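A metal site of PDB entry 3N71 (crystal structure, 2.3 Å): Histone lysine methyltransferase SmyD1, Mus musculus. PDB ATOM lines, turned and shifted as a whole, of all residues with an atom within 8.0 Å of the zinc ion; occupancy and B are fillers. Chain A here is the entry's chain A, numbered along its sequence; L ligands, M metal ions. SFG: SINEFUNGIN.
N of His 206 lies within hydrogen-bond range of N7 of the ligand.
O of His 206 is in hydrogen-bond range of N6 of the ligand, at 3.1 Å.
O of Cys 279 is in hydrogen-bond range of NH2 of Arg 263.
A ring nitrogen (NE2) of His 206 is in hydrogen-bond range of the backbone NH of Cys 208 (3.3 Å).
NE of Arg 263 is in hydrogen-bond range of O of Cys 274 (3.3 Å).
The side-chain sulfur (SG) of Cys 276 sits close to the side-chain carboxylate (OD1) of Asp 207 (3.6 Å).
The side-chain sulfur of Cys 208 lies close to the guanidinium group of Arg 262.
NE of Arg 262 lies within hydrogen-bond range of O of Phe 255, at 3.3 Å.
The side-chain sulfur (SG) of Cys 279 sits close to the guanidinium group (NH1) of Arg 262 (2.9 Å).
The side-chain sulfur (SG) of Cys 276 lies close to the backbone NH (N) of His 278, at 3.5 Å.
Residues that only touch the zinc ion: Arg 262.
Of the 20 residues printed, 5 come within 4 Å of the zinc ion.
The zinc ion is bound by the side-chain sulfur of Cys 274, the side-chain sulfur of Cys 279, the side-chain sulfur of Cys 276 and the side-chain sulfur of Cys 208.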
ATOM      1  N   HIS A 206       8.065   7.204 -20.396  1.00  0.00           N
ATOM      2  CA  HIS A 206       9.078   8.230 -20.532  1.00  0.00           C
ATOM      3  C   HIS A 206       8.604   9.670 -20.474  1.00  0.00           C
ATOM      4  O   HIS A 206       7.484  10.012 -20.839  1.00  0.00           O
ATOM      5  CB  HIS A 206       9.818   8.015 -21.861  1.00  0.00           C
ATOM      6  CG  HIS A 206      10.721   9.151 -22.233  1.00  0.00           C
ATOM      7  ND1 HIS A 206      12.013   9.253 -21.781  1.00  0.00           N
ATOM      8  CD2 HIS A 206      10.467  10.314 -22.897  1.00  0.00           C
ATOM      9  CE1 HIS A 206      12.513  10.429 -22.124  1.00  0.00           C
ATOM     10  NE2 HIS A 206      11.585  11.097 -22.804  1.00  0.00           N
ATOM     11  N   ASP A 207       9.503  10.531 -20.007  1.00  0.00           N
ATOM     12  CA  ASP A 207       9.283  11.971 -19.940  1.00  0.00           C
ATOM     13  C   ASP A 207      10.704  12.564 -19.892  1.00  0.00           C
ATOM     14  O   ASP A 207      11.549  12.109 -19.123  1.00  0.00           O
ATOM     15  CB  ASP A 207       8.499  12.357 -18.685  1.00  0.00           C
ATOM     16  CG  ASP A 207       8.017  13.809 -18.739  1.00  0.00           C
ATOM     17  OD1 ASP A 207       8.820  14.708 -19.070  1.00  0.00           O
ATOM     18  OD2 ASP A 207       6.824  14.051 -18.428  1.00  0.00           O
ATOM     19  N   CYS A 208      10.982  13.553 -20.733  1.00  0.00           N
ATOM     20  CA  CYS A 208      12.317  14.150 -20.744  1.00  0.00           C
ATOM     21  C   CYS A 208      12.724  14.843 -19.432  1.00  0.00           C
ATOM     22  O   CYS A 208      13.898  15.049 -19.159  1.00  0.00           O
ATOM     23  CB  CYS A 208      12.425  15.120 -21.920  1.00  0.00           C
ATOM     24  SG  CYS A 208      12.372  14.258 -23.493  1.00  0.00           S
ATOM     25  N   TRP A 209      11.734  15.194 -18.613  1.00  0.00           N
ATOM     26  CA  TRP A 209      11.959  15.828 -17.328  1.00  0.00           C
ATOM     27  C   TRP A 209      11.088  15.004 -16.377  1.00  0.00           C
ATOM     28  O   TRP A 209      10.040  15.446 -15.926  1.00  0.00           O
ATOM     29  CB  TRP A 209      11.486  17.278 -17.377  1.00  0.00           C
ATOM     30  CG  TRP A 209      11.880  18.137 -16.205  1.00  0.00           C
ATOM     31  CD1 TRP A 209      11.195  18.292 -15.038  1.00  0.00           C
ATOM     32  CD2 TRP A 209      13.057  18.954 -16.091  1.00  0.00           C
ATOM     33  NE1 TRP A 209      11.861  19.159 -14.196  1.00  0.00           N
ATOM     34  CE2 TRP A 209      13.011  19.573 -14.816  1.00  0.00           C
ATOM     35  CE3 TRP A 209      14.142  19.215 -16.930  1.00  0.00           C
ATOM     36  CZ2 TRP A 209      14.005  20.463 -14.380  1.00  0.00           C
ATOM     37  CZ3 TRP A 209      15.136  20.093 -16.500  1.00  0.00           C
ATOM     38  CH2 TRP A 209      15.065  20.699 -15.230  1.00  0.00           C
ATOM     39  N   SER A 251      13.341   8.990 -17.465  1.00  0.00           N
ATOM     40  CA  SER A 251      13.789   9.411 -18.782  1.00  0.00           C
ATOM     41  C   SER A 251      14.561   8.264 -19.398  1.00  0.00           C
ATOM     42  O   SER A 251      15.385   7.637 -18.741  1.00  0.00           O
ATOM     43  CB  SER A 251      14.678  10.648 -18.708  1.00  0.00           C
ATOM     44  OG  SER A 251      15.222  10.922 -19.986  1.00  0.00           O
ATOM     45  N   ILE A 253      16.401   8.694 -22.089  1.00  0.00           N
ATOM     46  CA  ILE A 253      17.610   9.241 -22.692  1.00  0.00           C
ATOM     47  C   ILE A 253      18.196  10.381 -21.886  1.00  0.00           C
ATOM     48  O   ILE A 253      17.646  10.780 -20.865  1.00  0.00           O
ATOM     49  CB  ILE A 253      17.318   9.756 -24.113  1.00  0.00           C
ATOM     50  CG1 ILE A 253      16.183  10.785 -24.065  1.00  0.00           C
ATOM     51  CG2 ILE A 253      16.950   8.588 -25.015  1.00  0.00           C
ATOM     52  CD1 ILE A 253      15.752  11.285 -25.432  1.00  0.00           C
ATOM     53  N   PHE A 255      19.044  14.176 -21.116  1.00  0.00           N
ATOM     54  CA  PHE A 255      18.332  15.411 -21.359  1.00  0.00           C
ATOM     55  C   PHE A 255      19.082  16.417 -22.235  1.00  0.00           C
ATOM     56  O   PHE A 255      18.451  17.192 -22.942  1.00  0.00           O
ATOM     57  CB  PHE A 255      17.984  16.058 -20.010  1.00  0.00           C
ATOM     58  CG  PHE A 255      17.108  17.269 -20.138  1.00  0.00           C
ATOM     59  CD1 PHE A 255      15.849  17.169 -20.716  1.00  0.00           C
ATOM     60  CD2 PHE A 255      17.566  18.513 -19.734  1.00  0.00           C
ATOM     61  CE1 PHE A 255      15.055  18.286 -20.900  1.00  0.00           C
ATOM     62  CE2 PHE A 255      16.788  19.646 -19.918  1.00  0.00           C
ATOM     63  CZ  PHE A 255      15.524  19.525 -20.501  1.00  0.00           C
ATOM     64  N   SER A 259      15.140  19.582 -28.061  1.00  0.00           N
ATOM     65  CA  SER A 259      13.883  18.829 -28.095  1.00  0.00           C
ATOM     66  C   SER A 259      13.786  18.050 -29.421  1.00  0.00           C
ATOM     67  O   SER A 259      13.455  16.862 -29.407  1.00  0.00           O
ATOM     68  CB  SER A 259      12.681  19.775 -27.951  1.00  0.00           C
ATOM     69  OG  SER A 259      12.818  20.935 -28.754  1.00  0.00           O
ATOM     70  N   ARG A 262      15.991  15.041 -29.144  1.00  0.00           N
ATOM     71  CA  ARG A 262      15.454  14.009 -28.264  1.00  0.00           C
ATOM     72  C   ARG A 262      14.332  13.242 -28.961  1.00  0.00           C
ATOM     73  O   ARG A 262      14.336  12.014 -28.957  1.00  0.00           O
ATOM     74  CB  ARG A 262      14.940  14.620 -26.956  1.00  0.00           C
ATOM     75  CG  ARG A 262      16.046  15.037 -26.001  1.00  0.00           C
ATOM     76  CD  ARG A 262      15.501  15.482 -24.651  1.00  0.00           C
ATOM     77  NE  ARG A 262      15.544  16.931 -24.517  1.00  0.00           N
ATOM     78  CZ  ARG A 262      14.483  17.725 -24.577  1.00  0.00           C
ATOM     79  NH1 ARG A 262      13.287  17.216 -24.752  1.00  0.00           N
ATOM     80  NH2 ARG A 262      14.642  19.037 -24.480  1.00  0.00           N
ATOM     81  N   ARG A 263      13.378  13.942 -29.549  1.00  0.00           N
ATOM     82  CA  ARG A 263      12.281  13.267 -30.237  1.00  0.00           C
ATOM     83  C   ARG A 263      12.784  12.272 -31.273  1.00  0.00           C
ATOM     84  O   ARG A 263      12.238  11.179 -31.416  1.00  0.00           O
ATOM     85  CB  ARG A 263      11.368  14.289 -30.902  1.00  0.00           C
ATOM     86  CG  ARG A 263      10.454  15.005 -29.932  1.00  0.00           C
ATOM     87  CD  ARG A 263       9.629  16.059 -30.631  1.00  0.00           C
ATOM     88  NE  ARG A 263       8.565  16.553 -29.760  1.00  0.00           N
ATOM     89  CZ  ARG A 263       7.740  17.544 -30.079  1.00  0.00           C
ATOM     90  NH1 ARG A 263       7.871  18.158 -31.254  1.00  0.00           N
ATOM     91  NH2 ARG A 263       6.798  17.926 -29.218  1.00  0.00           N
ATOM     92  N   LEU A 266      14.118   9.253 -29.379  1.00  0.00           N
ATOM     93  CA  LEU A 266      13.014   8.524 -28.776  1.00  0.00           C
ATOM     94  C   LEU A 266      12.202   7.806 -29.850  1.00  0.00           C
ATOM     95  O   LEU A 266      11.794   6.669 -29.657  1.00  0.00           O
ATOM     96  CB  LEU A 266      12.102   9.459 -27.984  1.00  0.00           C
ATOM     97  CG  LEU A 266      12.711   9.979 -26.695  1.00  0.00           C
ATOM     98  CD1 LEU A 266      11.772  10.982 -26.055  1.00  0.00           C
ATOM     99  CD2 LEU A 266      12.964   8.831 -25.752  1.00  0.00           C
ATOM    100  N   PHE A 272       7.976   6.209 -30.772  1.00  0.00           N
ATOM    101  CA  PHE A 272       6.917   7.100 -30.331  1.00  0.00           C
ATOM    102  C   PHE A 272       7.329   8.560 -30.420  1.00  0.00           C
ATOM    103  O   PHE A 272       8.509   8.871 -30.472  1.00  0.00           O
ATOM    104  CB  PHE A 272       6.452   6.766 -28.906  1.00  0.00           C
ATOM    105  CG  PHE A 272       7.342   7.274 -27.821  1.00  0.00           C
ATOM    106  CD1 PHE A 272       8.346   6.475 -27.277  1.00  0.00           C
ATOM    107  CD2 PHE A 272       7.170   8.557 -27.295  1.00  0.00           C
ATOM    108  CE1 PHE A 272       9.147   6.935 -26.232  1.00  0.00           C
ATOM    109  CE2 PHE A 272       7.963   9.020 -26.254  1.00  0.00           C
ATOM    110  CZ  PHE A 272       8.966   8.209 -25.717  1.00  0.00           C
ATOM    111  N   ASP A 273       6.330   9.439 -30.477  1.00  0.00           N
ATOM    112  CA  ASP A 273       6.588  10.881 -30.552  1.00  0.00           C
ATOM    113  C   ASP A 273       6.390  11.469 -29.166  1.00  0.00           C
ATOM    114  O   ASP A 273       5.273  11.580 -28.681  1.00  0.00           O
ATOM    115  CB  ASP A 273       5.630  11.549 -31.554  1.00  0.00           C
ATOM    116  CG  ASP A 273       5.613  10.863 -32.907  1.00  0.00           C
ATOM    117  OD1 ASP A 273       6.702  10.524 -33.416  1.00  0.00           O
ATOM    118  OD2 ASP A 273       4.495  10.674 -33.452  1.00  0.00           O
ATOM    119  N   CYS A 274       7.486  11.855 -28.525  1.00  0.00           N
ATOM    120  CA  CYS A 274       7.383  12.402 -27.187  1.00  0.00           C
ATOM    121  C   CYS A 274       6.550  13.683 -27.107  1.00  0.00           C
ATOM    122  O   CYS A 274       6.738  14.615 -27.881  1.00  0.00           O
ATOM    123  CB  CYS A 274       8.781  12.670 -26.631  1.00  0.00           C
ATOM    124  SG  CYS A 274       8.711  13.150 -24.910  1.00  0.00           S
ATOM    125  N   SER A 275       5.647  13.727 -26.132  1.00  0.00           N
ATOM    126  CA  SER A 275       4.782  14.881 -25.981  1.00  0.00           C
ATOM    127  C   SER A 275       4.862  15.490 -24.595  1.00  0.00           C
ATOM    128  O   SER A 275       3.889  16.101 -24.135  1.00  0.00           O
ATOM    129  CB  SER A 275       3.332  14.493 -26.270  1.00  0.00           C
ATOM    130  OG  SER A 275       2.906  13.524 -25.336  1.00  0.00           O
ATOM    131  N   CYS A 276       6.000  15.341 -23.921  1.00  0.00           N
ATOM    132  CA  CYS A 276       6.132  15.923 -22.607  1.00  0.00           C
ATOM    133  C   CYS A 276       6.184  17.448 -22.774  1.00  0.00           C
ATOM    134  O   CYS A 276       6.410  17.948 -23.867  1.00  0.00           O
ATOM    135  CB  CYS A 276       7.402  15.410 -21.897  1.00  0.00           C
ATOM    136  SG  CYS A 276       8.986  16.154 -22.417  1.00  0.00           S
ATOM    137  N   GLU A 277       5.970  18.158 -21.683  1.00  0.00           N
ATOM    138  CA  GLU A 277       5.968  19.611 -21.728  1.00  0.00           C
ATOM    139  C   GLU A 277       7.271  20.185 -22.271  1.00  0.00           C
ATOM    140  O   GLU A 277       7.258  21.183 -23.002  1.00  0.00           O
ATOM    141  CB  GLU A 277       5.714  20.173 -20.320  1.00  0.00           C
ATOM    142  CG  GLU A 277       5.646  21.680 -20.252  1.00  0.00           C
ATOM    143  CD  GLU A 277       5.159  22.188 -18.904  1.00  0.00           C
ATOM    144  OE1 GLU A 277       5.793  21.871 -17.873  1.00  0.00           O
ATOM    145  OE2 GLU A 277       4.128  22.899 -18.874  1.00  0.00           O
ATOM    146  N   HIS A 278       8.396  19.555 -21.940  1.00  0.00           N
ATOM    147  CA  HIS A 278       9.689  20.064 -22.392  1.00  0.00           C
ATOM    148  C   HIS A 278       9.876  19.989 -23.904  1.00  0.00           C
ATOM    149  O   HIS A 278      10.477  20.875 -24.506  1.00  0.00           O
ATOM    150  CB  HIS A 278      10.821  19.363 -21.652  1.00  0.00           C
ATOM    151  CG  HIS A 278      11.020  19.876 -20.261  1.00  0.00           C
ATOM    152  ND1 HIS A 278      12.007  20.778 -19.935  1.00  0.00           N
ATOM    153  CD2 HIS A 278      10.304  19.683 -19.118  1.00  0.00           C
ATOM    154  CE1 HIS A 278      11.907  21.119 -18.665  1.00  0.00           C
ATOM    155  NE2 HIS A 278      10.872  20.465 -18.144  1.00  0.00           N
ATOM    156  N   CYS A 279       9.356  18.928 -24.520  1.00  0.00           N
ATOM    157  CA  CYS A 279       9.461  18.768 -25.975  1.00  0.00           C
ATOM    158  C   CYS A 279       8.420  19.564 -26.761  1.00  0.00           C
ATOM    159  O   CYS A 279       8.710  20.021 -27.869  1.00  0.00           O
ATOM    160  CB  CYS A 279       9.344  17.289 -26.345  1.00  0.00           C
ATOM    161  SG  CYS A 279      10.875  16.391 -26.056  1.00  0.00           S
ATOM    162  N   GLN A 280       7.222  19.727 -26.203  1.00  0.00           N
ATOM    163  CA  GLN A 280       6.161  20.480 -26.867  1.00  0.00           C
ATOM    164  C   GLN A 280       6.398  21.979 -26.823  1.00  0.00           C
ATOM    165  O   GLN A 280       5.992  22.704 -27.718  1.00  0.00           O
ATOM    166  CB  GLN A 280       4.790  20.175 -26.251  1.00  0.00           C
ATOM    167  CG  GLN A 280       4.266  18.773 -26.539  1.00  0.00           C
ATOM    168  CD  GLN A 280       2.804  18.618 -26.191  1.00  0.00           C
ATOM    169  OE1 GLN A 280       2.377  18.978 -25.093  1.00  0.00           O
ATOM    170  NE2 GLN A 280       2.031  18.082 -27.114  1.00  0.00           N
HETATM  171  N   SFG L   1       3.508   1.885 -22.083  1.00  0.00           N
HETATM  172  CA  SFG L   1       4.256   0.607 -21.911  1.00  0.00           C
HETATM  173  C   SFG L   1       3.436  -0.710 -21.743  1.00  0.00           C
HETATM  174  O   SFG L   1       3.976  -1.765 -21.330  1.00  0.00           O
HETATM  175  OXT SFG L   1       2.230  -0.735 -22.020  1.00  0.00           O
HETATM  176  CB  SFG L   1       5.237   0.871 -20.729  1.00  0.00           C
HETATM  177  CG  SFG L   1       6.676   1.280 -21.140  1.00  0.00           C
HETATM  178  CD  SFG L   1       7.447   0.342 -22.137  1.00  0.00           C
HETATM  179  NE  SFG L   1       8.683  -0.151 -21.460  1.00  0.00           N
HETATM  180  C5' SFG L   1       7.987   0.959 -23.437  1.00  0.00           C
HETATM  181  C4' SFG L   1       7.030   1.582 -24.489  1.00  0.00           C
HETATM  182  O4' SFG L   1       6.028   2.494 -23.987  1.00  0.00           O
HETATM  183  C3' SFG L   1       7.747   2.399 -25.533  1.00  0.00           C
HETATM  184  O3' SFG L   1       8.428   1.590 -26.479  1.00  0.00           O
HETATM  185  C2' SFG L   1       6.644   3.236 -26.155  1.00  0.00           C
HETATM  186  O2' SFG L   1       5.969   2.499 -27.189  1.00  0.00           O
HETATM  187  C1' SFG L   1       5.752   3.522 -24.961  1.00  0.00           C
HETATM  188  N9  SFG L   1       5.999   4.862 -24.346  1.00  0.00           N
HETATM  189  C8  SFG L   1       6.869   5.155 -23.312  1.00  0.00           C
HETATM  190  N7  SFG L   1       6.865   6.416 -23.007  1.00  0.00           N
HETATM  191  C5  SFG L   1       5.933   7.004 -23.863  1.00  0.00           C
HETATM  192  C6  SFG L   1       5.464   8.357 -24.091  1.00  0.00           C
HETATM  193  N6  SFG L   1       5.845   9.448 -23.371  1.00  0.00           N
HETATM  194  N1  SFG L   1       4.506   8.595 -25.072  1.00  0.00           N
HETATM  195  C2  SFG L   1       4.088   7.539 -25.809  1.00  0.00           C
HETATM  196  N3  SFG L   1       4.459   6.238 -25.699  1.00  0.00           N
HETATM  197  C4  SFG L   1       5.416   6.042 -24.734  1.00  0.00           C
HETATM  198 ZN    ZN M   1      10.026  14.931 -24.387  1.00  0.00          ZN
